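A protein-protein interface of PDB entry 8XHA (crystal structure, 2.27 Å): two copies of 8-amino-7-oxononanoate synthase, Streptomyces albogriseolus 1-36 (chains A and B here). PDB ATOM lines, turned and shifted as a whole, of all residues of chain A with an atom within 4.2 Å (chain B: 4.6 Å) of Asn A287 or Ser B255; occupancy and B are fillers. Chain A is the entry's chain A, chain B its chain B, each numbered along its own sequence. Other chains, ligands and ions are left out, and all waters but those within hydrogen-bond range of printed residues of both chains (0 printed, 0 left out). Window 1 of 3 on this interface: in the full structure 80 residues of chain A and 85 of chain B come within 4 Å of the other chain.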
ATOM      1  N   LEU A  78      21.447   3.887 -29.688  1.00  0.00           N
ATOM      2  CA  LEU A  78      20.235   4.597 -29.284  1.00  0.00           C
ATOM      3  C   LEU A  78      18.975   3.967 -29.876  1.00  0.00           C
ATOM      4  O   LEU A  78      17.930   3.975 -29.219  1.00  0.00           O
ATOM      5  CB  LEU A  78      20.314   6.074 -29.661  1.00  0.00           C
ATOM      6  CG  LEU A  78      20.786   7.039 -28.565  1.00  0.00           C
ATOM      7  CD1 LEU A  78      20.794   8.428 -29.124  1.00  0.00           C
ATOM      8  CD2 LEU A  78      19.930   6.983 -27.297  1.00  0.00           C
ATOM      9  N   GLN A 284       9.812   7.290 -36.198  1.00  0.00           N
ATOM     10  CA  GLN A 284      10.822   6.565 -35.387  1.00  0.00           C
ATOM     11  C   GLN A 284      10.276   5.850 -34.160  1.00  0.00           C
ATOM     12  O   GLN A 284       9.405   6.398 -33.476  1.00  0.00           O
ATOM     13  CB  GLN A 284      11.944   7.519 -34.971  1.00  0.00           C
ATOM     14  CG  GLN A 284      11.479   8.845 -34.395  1.00  0.00           C
ATOM     15  CD  GLN A 284      12.661   9.734 -34.100  1.00  0.00           C
ATOM     16  OE1 GLN A 284      13.501   9.424 -33.260  1.00  0.00           O
ATOM     17  NE2 GLN A 284      12.743  10.850 -34.802  1.00  0.00           N
ATOM     18  N   ARG A 285      10.831   4.672 -33.906  1.00  0.00           N
ATOM     19  CA  ARG A 285      10.473   3.912 -32.699  1.00  0.00           C
ATOM     20  C   ARG A 285      11.126   4.601 -31.505  1.00  0.00           C
ATOM     21  O   ARG A 285      11.988   5.454 -31.718  1.00  0.00           O
ATOM     22  CB  ARG A 285      11.007   2.487 -32.850  1.00  0.00           C
ATOM     23  CG  ARG A 285      10.568   1.791 -34.128  1.00  0.00           C
ATOM     24  CD  ARG A 285      11.717   1.049 -34.780  1.00  0.00           C
ATOM     25  NE  ARG A 285      12.905   1.885 -34.863  1.00  0.00           N
ATOM     26  CZ  ARG A 285      13.116   2.804 -35.796  1.00  0.00           C
ATOM     27  NH1 ARG A 285      12.210   3.019 -36.732  1.00  0.00           N
ATOM     28  NH2 ARG A 285      14.231   3.511 -35.786  1.00  0.00           N
ATOM     29  N   LEU A 286      10.718   4.234 -30.303  1.00  0.00           N
ATOM     30  CA  LEU A 286      11.318   4.805 -29.080  1.00  0.00           C
ATOM     31  C   LEU A 286      12.774   4.347 -28.969  1.00  0.00           C
ATOM     32  O   LEU A 286      13.074   3.224 -29.393  1.00  0.00           O
ATOM     33  CB  LEU A 286      10.486   4.344 -27.884  1.00  0.00           C
ATOM     34  CG  LEU A 286       9.184   5.101 -27.646  1.00  0.00           C
ATOM     35  CD1 LEU A 286       8.327   4.382 -26.618  1.00  0.00           C
ATOM     36  CD2 LEU A 286       9.472   6.524 -27.199  1.00  0.00           C
ATOM     37  N   ASN A 287      13.633   5.196 -28.410  1.00  0.00           N
ATOM     38  CA  ASN A 287      15.043   4.864 -28.273  1.00  0.00           C
ATOM     39  C   ASN A 287      15.245   3.816 -27.167  1.00  0.00           C
ATOM     40  O   ASN A 287      14.350   3.507 -26.384  1.00  0.00           O
ATOM     41  CB  ASN A 287      15.888   6.132 -28.059  1.00  0.00           C
ATOM     42  CG  ASN A 287      15.605   6.868 -26.727  1.00  0.00           C
ATOM     43  OD1 ASN A 287      14.908   6.386 -25.837  1.00  0.00           O
ATOM     44  ND2 ASN A 287      16.191   8.048 -26.599  1.00  0.00           N
ATOM     45  N   THR A 288      16.429   3.235 -27.129  1.00  0.00           N
ATOM     46  CA  THR A 288      16.597   2.075 -26.251  1.00  0.00           C
ATOM     47  C   THR A 288      16.489   2.405 -24.762  1.00  0.00           C
ATOM     48  O   THR A 288      15.943   1.587 -24.012  1.00  0.00           O
ATOM     49  CB  THR A 288      17.924   1.359 -26.544  1.00  0.00           C
ATOM     50  OG1 THR A 288      19.010   2.287 -26.500  1.00  0.00           O
ATOM     51  CG2 THR A 288      17.880   0.702 -27.925  1.00  0.00           C
ATOM     52  N   PRO A 289      16.963   3.561 -24.270  1.00  0.00           N
ATOM     53  CA  PRO A 289      16.704   3.850 -22.848  1.00  0.00           C
ATOM     54  C   PRO A 289      15.213   3.945 -22.536  1.00  0.00           C
ATOM     55  O   PRO A 289      14.767   3.469 -21.482  1.00  0.00           O
ATOM     56  CB  PRO A 289      17.459   5.171 -22.606  1.00  0.00           C
ATOM     57  CG  PRO A 289      17.670   5.762 -23.952  1.00  0.00           C
ATOM     58  CD  PRO A 289      17.805   4.611 -24.890  1.00  0.00           C
ATOM     59  N   ALA A 290      14.420   4.504 -23.450  1.00  0.00           N
ATOM     60  CA  ALA A 290      12.976   4.529 -23.239  1.00  0.00           C
ATOM     61  C   ALA A 290      12.407   3.120 -23.142  1.00  0.00           C
ATOM     62  O   ALA A 290      11.555   2.840 -22.287  1.00  0.00           O
ATOM     63  CB  ALA A 290      12.299   5.313 -24.372  1.00  0.00           C
ATOM     64  N   LEU A 291      12.863   2.210 -24.009  1.00  0.00           N
ATOM     65  CA  LEU A 291      12.329   0.850 -23.974  1.00  0.00           C
ATOM     66  C   LEU A 291      12.761   0.127 -22.709  1.00  0.00           C
ATOM     67  O   LEU A 291      11.958  -0.584 -22.089  1.00  0.00           O
ATOM     68  CB  LEU A 291      12.764   0.072 -25.221  1.00  0.00           C
ATOM     69  CG  LEU A 291      12.237   0.670 -26.528  1.00  0.00           C
ATOM     70  CD1 LEU A 291      12.957   0.101 -27.751  1.00  0.00           C
ATOM     71  CD2 LEU A 291      10.725   0.476 -26.638  1.00  0.00           C
ATOM     72  N   LEU B 248      16.580  13.599 -36.420  1.00  0.00           N
ATOM     73  CA  LEU B 248      17.935  13.560 -35.823  1.00  0.00           C
ATOM     74  C   LEU B 248      18.301  12.117 -35.490  1.00  0.00           C
ATOM     75  O   LEU B 248      19.329  11.924 -34.843  1.00  0.00           O
ATOM     76  CB  LEU B 248      17.926  14.427 -34.564  1.00  0.00           C
ATOM     77  CG  LEU B 248      17.572  15.898 -34.765  1.00  0.00           C
ATOM     78  CD1 LEU B 248      17.420  16.600 -33.426  1.00  0.00           C
ATOM     79  CD2 LEU B 248      18.619  16.595 -35.616  1.00  0.00           C
ATOM     80  N   ASN B 249      17.492  11.157 -35.938  1.00  0.00           N
ATOM     81  CA  ASN B 249      17.730   9.724 -35.627  1.00  0.00           C
ATOM     82  C   ASN B 249      18.406   9.030 -36.809  1.00  0.00           C
ATOM     83  O   ASN B 249      18.585   7.810 -36.745  1.00  0.00           O
ATOM     84  CB  ASN B 249      16.441   8.994 -35.243  1.00  0.00           C
ATOM     85  CG  ASN B 249      15.611   8.540 -36.423  1.00  0.00           C
ATOM     86  OD1 ASN B 249      15.303   9.325 -37.313  1.00  0.00           O
ATOM     87  ND2 ASN B 249      15.227   7.275 -36.424  1.00  0.00           N
ATOM     88  N   ALA B 254      21.320  10.767 -33.231  1.00  0.00           N
ATOM     89  CA  ALA B 254      20.621  10.922 -31.944  1.00  0.00           C
ATOM     90  C   ALA B 254      19.194  10.404 -32.080  1.00  0.00           C
ATOM     91  O   ALA B 254      19.004   9.354 -32.701  1.00  0.00           O
ATOM     92  CB  ALA B 254      20.653  12.361 -31.519  1.00  0.00           C
ATOM     93  N   SER B 255      18.242  11.118 -31.492  1.00  0.00           N
ATOM     94  CA  SER B 255      16.823  10.712 -31.558  1.00  0.00           C
ATOM     95  C   SER B 255      15.961  11.963 -31.702  1.00  0.00           C
ATOM     96  O   SER B 255      16.427  13.045 -31.337  1.00  0.00           O
ATOM     97  CB  SER B 255      16.439   9.913 -30.346  1.00  0.00           C
ATOM     98  OG  SER B 255      17.235   8.749 -30.222  1.00  0.00           O
ATOM     99  N   GLY B 256      14.759  11.799 -32.230  1.00  0.00           N
ATOM    100  CA  GLY B 256      13.827  12.927 -32.312  1.00  0.00           C
ATOM    101  C   GLY B 256      13.920  13.691 -33.606  1.00  0.00           C
ATOM    102  O   GLY B 256      14.499  13.172 -34.564  1.00  0.00           O
ATOM    103  N   GLY B 257      13.344  14.885 -33.616  1.00  0.00           N
ATOM    104  CA  GLY B 257      13.366  15.735 -34.811  1.00  0.00           C
ATOM    105  C   GLY B 257      13.551  17.181 -34.430  1.00  0.00           C
ATOM    106  O   GLY B 257      13.824  17.451 -33.259  1.00  0.00           O
ATOM    107  N   LEU B 286      11.908  15.527 -25.988  1.00  0.00           N
ATOM    108  CA  LEU B 286      12.874  14.433 -26.031  1.00  0.00           C
ATOM    109  C   LEU B 286      13.393  14.133 -24.633  1.00  0.00           C
ATOM    110  O   LEU B 286      13.602  15.052 -23.837  1.00  0.00           O
ATOM    111  CB  LEU B 286      14.032  14.820 -26.941  1.00  0.00           C
ATOM    112  CG  LEU B 286      13.820  14.705 -28.447  1.00  0.00           C
ATOM    113  CD1 LEU B 286      14.938  15.419 -29.170  1.00  0.00           C
ATOM    114  CD2 LEU B 286      13.822  13.242 -28.809  1.00  0.00           C
ATOM    115  N   ASN B 287      13.598  12.841 -24.328  1.00  0.00           N
ATOM    116  CA  ASN B 287      14.119  12.440 -23.024  1.00  0.00           C
ATOM    117  C   ASN B 287      15.609  12.788 -22.911  1.00  0.00           C
ATOM    118  O   ASN B 287      16.271  13.139 -23.893  1.00  0.00           O
ATOM    119  CB  ASN B 287      13.851  10.950 -22.745  1.00  0.00           C
ATOM    120  CG  ASN B 287      14.589   9.992 -23.691  1.00  0.00           C
ATOM    121  OD1 ASN B 287      15.504  10.367 -24.417  1.00  0.00           O
ATOM    122  ND2 ASN B 287      14.170   8.738 -23.672  1.00  0.00           N
ATOM    123  N   ALA B 290      18.444  11.269 -25.141  1.00  0.00           N
ATOM    124  CA  ALA B 290      18.417  11.820 -26.488  1.00  0.00           C
ATOM    125  C   ALA B 290      19.015  13.218 -26.516  1.00  0.00           C
ATOM    126  O   ALA B 290      19.764  13.560 -27.442  1.00  0.00           O
ATOM    127  CB  ALA B 290      16.980  11.832 -27.028  1.00  0.00           C
ATOM    128  N   ILE B 294      22.215  14.532 -28.641  1.00  0.00           N
ATOM    129  CA  ILE B 294      22.172  15.676 -29.548  1.00  0.00           C
ATOM    130  C   ILE B 294      23.349  16.606 -29.289  1.00  0.00           C
ATOM    131  O   ILE B 294      24.019  17.057 -30.223  1.00  0.00           O
ATOM    132  CB  ILE B 294      20.824  16.411 -29.412  1.00  0.00           C
ATOM    133  CG1 ILE B 294      19.699  15.547 -29.984  1.00  0.00           C
ATOM    134  CG2 ILE B 294      20.879  17.789 -30.034  1.00  0.00           C
ATOM    135  CD1 ILE B 294      18.323  16.166 -29.874  1.00  0.00           C
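Of the 9 printed residues of chain A, 5 touch a printed residue of chain B.
Hydrophobic or aromatic side chains of chain A within 4 Å of the printed part of chain B: Leu A78 and Ala A290.
Of the 10 printed residues of chain B, 6 touch a printed residue of chain A.
Printed residues of chain B that touch a printed residue of chain A: Asn B249, Ala B254, Ser B255, Gly B256, Asn B287 and Ala B290.
Among the printed residues, 10 pairs touch across the chains.
Asn B287 touches its own counterpart, Asn A287.
Asn A287 touches Ala B290, and with the chains exchanged Ala A290 touches Asn B287.
Positions printed for both chains: 286, 287 and 290.
Of the 10 pairs that touch across the chains among the printed residues, 3 have their exchanged pair printed and touching as well.
CD1 of Leu A78 touches CA of Ala B254 (3.8 Å).
Ser B255 touches Leu A78 (OG to CD1, 3.7 Å).
CB of Asn B249 touches OE1 of Gln A284, at 3.6 Å.
Ser B255 touches Gln A284.
Asn B249 touches Arg A285 (ND2 to NH2, 3.9 Å).
CB of Asn A287 touches OG of Ser B255, 3.7 Å away.
CB of Ala B290 touches ND2 of Asn A287, at 3.9 Å.
ND2 of Asn B287 touches CB of Ala A290 (3.97 Å).
The side-chain amide oxygen (OD1) of Asn A287 is in hydrogen-bond range of the backbone NH (N) of Ala A290, at 3.1 Å.
The backbone carbonyl oxygen (O) of Leu B248 sits at hydrogen-bond distance from the backbone NH (N) of Ala B254 (2.8 Å).
The backbone carbonyl oxygen (O) of Gly B256 sits at hydrogen-bond distance from the backbone NH (N) of Leu B248.
The backbone carbonyl oxygen (O) of Leu A78 is in hydrogen-bond range of the backbone NH (N) of Thr A288 (2.7 Å).
The backbone NH (N) of Ala B290 is in hydrogen-bond range of the side-chain amide oxygen (OD1) of Asn B287, 3.2 Å away.
OD1 of Asn B287 is in hydrogen-bond range of ND2 of Asn A287 (3.3 Å).
OE1 of Gln A284 is in hydrogen-bond range of N of Gly B256, at 2.9 Å.
Of the printed residues of chain B, Gln A284 touches Asn B249 (3.6 Å), Ser B255 (3.9 Å) and Gly B256 (2.9 Å).
Asn A287 touches just these residues of chain B: Ser B255, Asn B287 and Ala B290.
Ser B255 touches just these residues of chain A: Leu A78, Gln A284 and Asn A287.
Printed residues of chain A within 4 Å of Gly B256: Gln A284 (2.9 Å).
The nearest printed residue of chain B that does not touch Asn A287 is Leu B286 (6.1 Å).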
